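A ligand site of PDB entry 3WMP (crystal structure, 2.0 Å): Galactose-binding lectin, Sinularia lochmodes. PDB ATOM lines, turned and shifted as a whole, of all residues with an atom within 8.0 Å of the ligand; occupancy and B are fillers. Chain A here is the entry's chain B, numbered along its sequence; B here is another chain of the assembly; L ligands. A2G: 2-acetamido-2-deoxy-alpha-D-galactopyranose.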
ATOM      1  N   ASN A  55      36.447 -28.023  -4.208  1.00  0.00           N
ATOM      2  CA  ASN A  55      35.032 -28.308  -4.450  1.00  0.00           C
ATOM      3  C   ASN A  55      34.787 -28.409  -5.955  1.00  0.00           C
ATOM      4  O   ASN A  55      35.697 -28.173  -6.748  1.00  0.00           O
ATOM      5  CB  ASN A  55      34.129 -27.249  -3.804  1.00  0.00           C
ATOM      6  CG  ASN A  55      34.128 -27.348  -2.282  1.00  0.00           C
ATOM      7  OD1 ASN A  55      33.641 -28.314  -1.707  1.00  0.00           O
ATOM      8  ND2 ASN A  55      34.693 -26.340  -1.625  1.00  0.00           N
ATOM      9  N   ASN A  56      33.576 -28.789  -6.347  1.00  0.00           N
ATOM     10  CA  ASN A  56      33.248 -28.930  -7.763  1.00  0.00           C
ATOM     11  C   ASN A  56      33.350 -27.614  -8.518  1.00  0.00           C
ATOM     12  O   ASN A  56      33.184 -26.547  -7.943  1.00  0.00           O
ATOM     13  CB  ASN A  56      31.817 -29.493  -7.917  1.00  0.00           C
ATOM     14  CG  ASN A  56      31.754 -30.976  -7.656  1.00  0.00           C
ATOM     15  OD1 ASN A  56      32.777 -31.622  -7.411  1.00  0.00           O
ATOM     16  ND2 ASN A  56      30.546 -31.540  -7.707  1.00  0.00           N
ATOM     17  N   LEU A  57      33.643 -27.698  -9.820  1.00  0.00           N
ATOM     18  CA  LEU A  57      33.698 -26.508 -10.644  1.00  0.00           C
ATOM     19  C   LEU A  57      32.294 -26.202 -11.161  1.00  0.00           C
ATOM     20  O   LEU A  57      31.725 -26.966 -11.940  1.00  0.00           O
ATOM     21  CB  LEU A  57      34.640 -26.704 -11.848  1.00  0.00           C
ATOM     22  CG  LEU A  57      34.860 -25.477 -12.767  1.00  0.00           C
ATOM     23  CD1 LEU A  57      36.308 -25.451 -13.260  1.00  0.00           C
ATOM     24  CD2 LEU A  57      33.908 -25.497 -13.941  1.00  0.00           C
ATOM     25  N   ARG A  58      31.728 -25.091 -10.709  1.00  0.00           N
ATOM     26  CA  ARG A  58      30.409 -24.676 -11.163  1.00  0.00           C
ATOM     27  C   ARG A  58      30.455 -23.224 -11.644  1.00  0.00           C
ATOM     28  O   ARG A  58      30.586 -22.311 -10.841  1.00  0.00           O
ATOM     29  CB  ARG A  58      29.365 -24.800 -10.034  1.00  0.00           C
ATOM     30  CG  ARG A  58      29.218 -26.206  -9.475  1.00  0.00           C
ATOM     31  CD  ARG A  58      28.400 -26.199  -8.183  1.00  0.00           C
ATOM     32  NE  ARG A  58      28.349 -27.517  -7.553  1.00  0.00           N
ATOM     33  CZ  ARG A  58      29.079 -27.879  -6.500  1.00  0.00           C
ATOM     34  NH1 ARG A  58      29.937 -27.012  -5.955  1.00  0.00           N
ATOM     35  NH2 ARG A  58      28.962 -29.095  -5.995  1.00  0.00           N
ATOM     36  N   SER A  77      28.409 -18.495 -10.027  1.00  0.00           N
ATOM     37  CA  SER A  77      28.776 -19.852  -9.613  1.00  0.00           C
ATOM     38  C   SER A  77      27.611 -20.198  -8.658  1.00  0.00           C
ATOM     39  O   SER A  77      26.668 -19.411  -8.504  1.00  0.00           O
ATOM     40  CB  SER A  77      30.086 -19.917  -8.838  1.00  0.00           C
ATOM     41  OG  SER A  77      30.166 -18.905  -7.852  1.00  0.00           O
ATOM     42  N   TRP A  78      27.649 -21.382  -8.037  1.00  0.00           N
ATOM     43  CA  TRP A  78      26.618 -21.752  -7.078  1.00  0.00           C
ATOM     44  C   TRP A  78      27.101 -22.843  -6.116  1.00  0.00           C
ATOM     45  O   TRP A  78      28.150 -23.472  -6.340  1.00  0.00           O
ATOM     46  CB  TRP A  78      25.318 -22.148  -7.777  1.00  0.00           C
ATOM     47  CG  TRP A  78      25.374 -23.394  -8.611  1.00  0.00           C
ATOM     48  CD1 TRP A  78      24.985 -24.647  -8.228  1.00  0.00           C
ATOM     49  CD2 TRP A  78      25.863 -23.511  -9.952  1.00  0.00           C
ATOM     50  NE1 TRP A  78      25.182 -25.536  -9.257  1.00  0.00           N
ATOM     51  CE2 TRP A  78      25.718 -24.873 -10.327  1.00  0.00           C
ATOM     52  CE3 TRP A  78      26.400 -22.615 -10.877  1.00  0.00           C
ATOM     53  CZ2 TRP A  78      26.102 -25.345 -11.580  1.00  0.00           C
ATOM     54  CZ3 TRP A  78      26.774 -23.086 -12.127  1.00  0.00           C
ATOM     55  CH2 TRP A  78      26.629 -24.435 -12.468  1.00  0.00           C
ATOM     56  N   TYR A  79      26.332 -23.058  -5.060  1.00  0.00           N
ATOM     57  CA  TYR A  79      26.640 -24.007  -4.009  1.00  0.00           C
ATOM     58  C   TYR A  79      28.023 -23.743  -3.399  1.00  0.00           C
ATOM     59  O   TYR A  79      28.341 -22.612  -3.052  1.00  0.00           O
ATOM     60  CB  TYR A  79      26.506 -25.466  -4.482  1.00  0.00           C
ATOM     61  CG  TYR A  79      26.397 -26.457  -3.351  1.00  0.00           C
ATOM     62  CD1 TYR A  79      25.430 -26.298  -2.357  1.00  0.00           C
ATOM     63  CD2 TYR A  79      27.244 -27.553  -3.272  1.00  0.00           C
ATOM     64  CE1 TYR A  79      25.316 -27.204  -1.313  1.00  0.00           C
ATOM     65  CE2 TYR A  79      27.137 -28.468  -2.235  1.00  0.00           C
ATOM     66  CZ  TYR A  79      26.179 -28.289  -1.255  1.00  0.00           C
ATOM     67  OH  TYR A  79      26.061 -29.183  -0.226  1.00  0.00           O
ATOM     68  N   THR A  80      28.871 -24.769  -3.332  1.00  0.00           N
ATOM     69  CA  THR A  80      30.146 -24.644  -2.624  1.00  0.00           C
ATOM     70  C   THR A  80      31.351 -24.273  -3.430  1.00  0.00           C
ATOM     71  O   THR A  80      32.473 -24.258  -2.923  1.00  0.00           O
ATOM     72  CB  THR A  80      30.475 -25.998  -1.911  1.00  0.00           C
ATOM     73  OG1 THR A  80      30.359 -27.074  -2.861  1.00  0.00           O
ATOM     74  CG2 THR A  80      29.524 -26.255  -0.747  1.00  0.00           C
ATOM     75  N   THR A  81      31.136 -23.935  -4.683  1.00  0.00           N
ATOM     76  CA  THR A  81      32.246 -23.611  -5.567  1.00  0.00           C
ATOM     77  C   THR A  81      32.994 -22.342  -5.195  1.00  0.00           C
ATOM     78  O   THR A  81      32.388 -21.373  -4.739  1.00  0.00           O
ATOM     79  CB  THR A  81      31.715 -23.498  -7.032  1.00  0.00           C
ATOM     80  OG1 THR A  81      31.403 -24.811  -7.512  1.00  0.00           O
ATOM     81  CG2 THR A  81      32.747 -22.840  -7.944  1.00  0.00           C
ATOM     82  N   TRP B  18      22.120 -33.294 -13.540  1.00  0.00           N
ATOM     83  CA  TRP B  18      22.028 -33.499 -12.101  1.00  0.00           C
ATOM     84  C   TRP B  18      20.590 -33.827 -11.693  1.00  0.00           C
ATOM     85  O   TRP B  18      19.659 -33.170 -12.150  1.00  0.00           O
ATOM     86  CB  TRP B  18      22.494 -32.219 -11.375  1.00  0.00           C
ATOM     87  CG  TRP B  18      22.330 -32.278  -9.890  1.00  0.00           C
ATOM     88  CD1 TRP B  18      21.289 -31.775  -9.157  1.00  0.00           C
ATOM     89  CD2 TRP B  18      23.234 -32.864  -8.949  1.00  0.00           C
ATOM     90  NE1 TRP B  18      21.487 -32.013  -7.828  1.00  0.00           N
ATOM     91  CE2 TRP B  18      22.673 -32.678  -7.667  1.00  0.00           C
ATOM     92  CE3 TRP B  18      24.452 -33.530  -9.070  1.00  0.00           C
ATOM     93  CZ2 TRP B  18      23.309 -33.135  -6.513  1.00  0.00           C
ATOM     94  CZ3 TRP B  18      25.088 -33.973  -7.919  1.00  0.00           C
ATOM     95  CH2 TRP B  18      24.503 -33.782  -6.654  1.00  0.00           C
ATOM     96  N   PRO B  19      20.408 -34.804 -10.774  1.00  0.00           N
ATOM     97  CA  PRO B  19      21.411 -35.622 -10.072  1.00  0.00           C
ATOM     98  C   PRO B  19      22.013 -36.771 -10.860  1.00  0.00           C
ATOM     99  O   PRO B  19      22.768 -37.563 -10.289  1.00  0.00           O
ATOM    100  CB  PRO B  19      20.686 -36.076  -8.823  1.00  0.00           C
ATOM    101  CG  PRO B  19      19.305 -36.284  -9.318  1.00  0.00           C
ATOM    102  CD  PRO B  19      19.051 -35.197 -10.355  1.00  0.00           C
ATOM    103  N   ARG B  20      21.633 -36.911 -12.114  1.00  0.00           N
ATOM    104  CA  ARG B  20      22.290 -37.922 -12.926  1.00  0.00           C
ATOM    105  C   ARG B  20      23.505 -37.284 -13.601  1.00  0.00           C
ATOM    106  O   ARG B  20      23.598 -36.057 -13.716  1.00  0.00           O
ATOM    107  CB  ARG B  20      21.391 -38.369 -14.108  1.00  0.00           C
ATOM    108  CG  ARG B  20      19.925 -38.646 -13.783  1.00  0.00           C
ATOM    109  CD  ARG B  20      19.213 -39.233 -15.006  1.00  0.00           C
ATOM    110  NE  ARG B  20      17.873 -39.711 -14.702  1.00  0.00           N
ATOM    111  CZ  ARG B  20      16.810 -38.933 -14.530  1.00  0.00           C
ATOM    112  NH1 ARG B  20      16.932 -37.619 -14.637  1.00  0.00           N
ATOM    113  NH2 ARG B  20      15.626 -39.468 -14.250  1.00  0.00           N
ATOM    114  N   LEU B  49      29.208 -24.713 -16.969  1.00  0.00           N
ATOM    115  CA  LEU B  49      29.873 -25.989 -16.707  1.00  0.00           C
ATOM    116  C   LEU B  49      29.837 -26.418 -15.231  1.00  0.00           C
ATOM    117  O   LEU B  49      30.068 -25.619 -14.331  1.00  0.00           O
ATOM    118  CB  LEU B  49      31.320 -25.901 -17.218  1.00  0.00           C
ATOM    119  CG  LEU B  49      32.092 -27.189 -17.464  1.00  0.00           C
ATOM    120  CD1 LEU B  49      31.295 -28.126 -18.361  1.00  0.00           C
ATOM    121  CD2 LEU B  49      33.422 -26.841 -18.099  1.00  0.00           C
ATOM    122  N   ASP B  50      29.542 -27.700 -15.002  1.00  0.00           N
ATOM    123  CA  ASP B  50      29.455 -28.280 -13.649  1.00  0.00           C
ATOM    124  C   ASP B  50      30.195 -29.602 -13.688  1.00  0.00           C
ATOM    125  O   ASP B  50      29.652 -30.610 -14.137  1.00  0.00           O
ATOM    126  CB  ASP B  50      27.974 -28.484 -13.280  1.00  0.00           C
ATOM    127  CG  ASP B  50      27.782 -28.933 -11.848  1.00  0.00           C
ATOM    128  OD1 ASP B  50      26.627 -28.846 -11.370  1.00  0.00           O
ATOM    129  OD2 ASP B  50      28.758 -29.369 -11.188  1.00  0.00           O
ATOM    130  N   VAL B  51      31.446 -29.588 -13.208  1.00  0.00           N
ATOM    131  CA  VAL B  51      32.312 -30.774 -13.274  1.00  0.00           C
ATOM    132  C   VAL B  51      32.814 -31.215 -11.916  1.00  0.00           C
ATOM    133  O   VAL B  51      33.354 -30.415 -11.143  1.00  0.00           O
ATOM    134  CB  VAL B  51      33.522 -30.482 -14.201  1.00  0.00           C
ATOM    135  CG1 VAL B  51      34.462 -31.669 -14.220  1.00  0.00           C
ATOM    136  CG2 VAL B  51      33.046 -30.134 -15.632  1.00  0.00           C
ATOM    137  N   ASP B  52      32.660 -32.502 -11.620  1.00  0.00           N
ATOM    138  CA  ASP B  52      33.074 -33.054 -10.339  1.00  0.00           C
ATOM    139  C   ASP B  52      34.575 -33.022 -10.135  1.00  0.00           C
ATOM    140  O   ASP B  52      35.348 -33.375 -11.030  1.00  0.00           O
ATOM    141  CB  ASP B  52      32.558 -34.491 -10.202  1.00  0.00           C
ATOM    142  CG  ASP B  52      32.422 -34.911  -8.760  1.00  0.00           C
ATOM    143  OD1 ASP B  52      33.445 -35.324  -8.169  1.00  0.00           O
ATOM    144  OD2 ASP B  52      31.298 -34.810  -8.204  1.00  0.00           O
ATOM    145  N   ASN B  53      35.010 -32.607  -8.942  1.00  0.00           N
ATOM    146  CA  ASN B  53      36.428 -32.512  -8.638  1.00  0.00           C
ATOM    147  C   ASN B  53      37.087 -33.853  -8.260  1.00  0.00           C
ATOM    148  O   ASN B  53      38.302 -33.909  -8.062  1.00  0.00           O
ATOM    149  CB  ASN B  53      36.652 -31.511  -7.489  1.00  0.00           C
ATOM    150  CG  ASN B  53      36.112 -32.011  -6.148  1.00  0.00           C
ATOM    151  OD1 ASN B  53      35.392 -33.010  -6.076  1.00  0.00           O
ATOM    152  ND2 ASN B  53      36.451 -31.301  -5.084  1.00  0.00           N
ATOM    153  N   THR B  82      33.471 -36.762 -14.434  1.00  0.00           N
ATOM    154  CA  THR B  82      32.044 -36.732 -14.156  1.00  0.00           C
ATOM    155  C   THR B  82      31.500 -35.311 -14.349  1.00  0.00           C
ATOM    156  O   THR B  82      31.861 -34.393 -13.615  1.00  0.00           O
ATOM    157  CB  THR B  82      31.704 -37.187 -12.736  1.00  0.00           C
ATOM    158  OG1 THR B  82      32.098 -38.560 -12.578  1.00  0.00           O
ATOM    159  CG2 THR B  82      30.206 -37.052 -12.479  1.00  0.00           C
ATOM    160  N   VAL B  83      30.646 -35.138 -15.353  1.00  0.00           N
ATOM    161  CA  VAL B  83      30.040 -33.839 -15.634  1.00  0.00           C
ATOM    162  C   VAL B  83      28.579 -33.866 -15.190  1.00  0.00           C
ATOM    163  O   VAL B  83      27.853 -34.814 -15.481  1.00  0.00           O
ATOM    164  CB  VAL B  83      30.132 -33.510 -17.146  1.00  0.00           C
ATOM    165  CG1 VAL B  83      29.567 -32.123 -17.409  1.00  0.00           C
ATOM    166  CG2 VAL B  83      31.589 -33.588 -17.616  1.00  0.00           C
ATOM    167  N   TRP B  84      28.150 -32.839 -14.464  1.00  0.00           N
ATOM    168  CA  TRP B  84      26.781 -32.766 -13.927  1.00  0.00           C
ATOM    169  C   TRP B  84      25.825 -31.884 -14.705  1.00  0.00           C
ATOM    170  O   TRP B  84      24.620 -32.164 -14.774  1.00  0.00           O
ATOM    171  CB  TRP B  84      26.840 -32.298 -12.480  1.00  0.00           C
ATOM    172  CG  TRP B  84      27.507 -33.257 -11.560  1.00  0.00           C
ATOM    173  CD1 TRP B  84      28.671 -33.078 -10.892  1.00  0.00           C
ATOM    174  CD2 TRP B  84      27.033 -34.564 -11.212  1.00  0.00           C
ATOM    175  NE1 TRP B  84      28.968 -34.186 -10.130  1.00  0.00           N
ATOM    176  CE2 TRP B  84      27.971 -35.122 -10.307  1.00  0.00           C
ATOM    177  CE3 TRP B  84      25.911 -35.327 -11.563  1.00  0.00           C
ATOM    178  CZ2 TRP B  84      27.819 -36.394  -9.761  1.00  0.00           C
ATOM    179  CZ3 TRP B  84      25.761 -36.591 -11.012  1.00  0.00           C
ATOM    180  CH2 TRP B  84      26.708 -37.116 -10.122  1.00  0.00           C
ATOM    181  N   ASN B  85      26.357 -30.799 -15.253  1.00  0.00           N
ATOM    182  CA  ASN B  85      25.589 -29.871 -16.074  1.00  0.00           C
ATOM    183  C   ASN B  85      26.532 -29.181 -17.057  1.00  0.00           C
ATOM    184  O   ASN B  85      27.739 -29.084 -16.808  1.00  0.00           O
ATOM    185  CB  ASN B  85      24.953 -28.771 -15.201  1.00  0.00           C
ATOM    186  CG  ASN B  85      23.936 -29.317 -14.223  1.00  0.00           C
ATOM    187  OD1 ASN B  85      22.829 -29.713 -14.610  1.00  0.00           O
ATOM    188  ND2 ASN B  85      24.301 -29.351 -12.942  1.00  0.00           N
HETATM  189  O5  A2G L   1      26.264 -30.067  -6.588  1.00  0.00           O
HETATM  190  C1  A2G L   1      25.201 -29.626  -5.721  1.00  0.00           C
HETATM  191  O1  A2G L   1      24.427 -30.729  -5.387  1.00  0.00           O
HETATM  192  C2  A2G L   1      24.330 -28.579  -6.408  1.00  0.00           C
HETATM  193  N2  A2G L   1      23.190 -28.291  -5.561  1.00  0.00           N
HETATM  194  C3  A2G L   1      23.836 -29.101  -7.768  1.00  0.00           C
HETATM  195  O3  A2G L   1      23.158 -28.068  -8.467  1.00  0.00           O
HETATM  196  C4  A2G L   1      25.005 -29.597  -8.610  1.00  0.00           C
HETATM  197  O4  A2G L   1      25.854 -28.509  -8.931  1.00  0.00           O
HETATM  198  C5  A2G L   1      25.778 -30.653  -7.820  1.00  0.00           C
HETATM  199  C6  A2G L   1      26.966 -31.233  -8.564  1.00  0.00           C
HETATM  200  O6  A2G L   1      28.049 -30.324  -8.651  1.00  0.00           O
HETATM  201  C7  A2G L   1      22.875 -27.046  -5.214  1.00  0.00           C
HETATM  202  O7  A2G L   1      23.502 -26.051  -5.609  1.00  0.00           O
HETATM  203  C8  A2G L   1      21.684 -26.872  -4.289  1.00  0.00           C
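The side-chain carboxylate (OD1) of Asp 50 of chain B sits at hydrogen-bond distance from an oxygen (O4) of the ligand, 2.6 Å away.
The guanidinium group of Arg 58 lies within hydrogen-bond range of an oxygen (O5) of the ligand.
The side-chain amide nitrogen of Asn 56 sits at hydrogen-bond distance from an oxygen (O6) of the ligand.
O4 of the ligand is in hydrogen-bond range of NE1 of Trp 78 (3.1 Å).
Merely in contact with the ligand: Trp 18 of chain B (2.9 Å), Tyr 79 (3.3 Å) and Trp 84 of chain B (3.4 Å).
Hydrophobic or aromatic side chains that line the ligand: Trp 78, Tyr 79, Trp 18 of chain B and Trp 84 of chain B.
The nearest printed residue that does not touch the ligand is Asn 85 of chain B (4.4 Å).
The backbone carbonyl oxygen of Asp 50 of chain B lies within hydrogen-bond range of the backbone NH of Trp 84 of chain B.
The side-chain amide nitrogen (ND2) of Asn 85 of chain B lies within hydrogen-bond range of the side-chain carboxylate (OD1) of Asp 50 of chain B (2.9 Å).
The guanidinium group of Arg 58 sits close to the side-chain amide nitrogen of Asn 56.
NH1 of Arg 58 lies within hydrogen-bond range of OG1 of Thr 80 (3.1 Å).
The side-chain hydroxyl (OG1) of Thr 81 sits at hydrogen-bond distance from the guanidinium group (NH1) of Arg 58 (3.1 Å).
The backbone carbonyl oxygen (O) of Asn 56 sits at hydrogen-bond distance from the side-chain hydroxyl (OG1) of Thr 81 (2.5 Å).
The side-chain amide oxygen (OD1) of Asn 56 is in hydrogen-bond range of the backbone NH (N) of Asn 53 of chain B (2.9 Å).
NE1 of Trp 84 of chain B sits at hydrogen-bond distance from OD2 of Asp 52 of chain B (3.1 Å).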
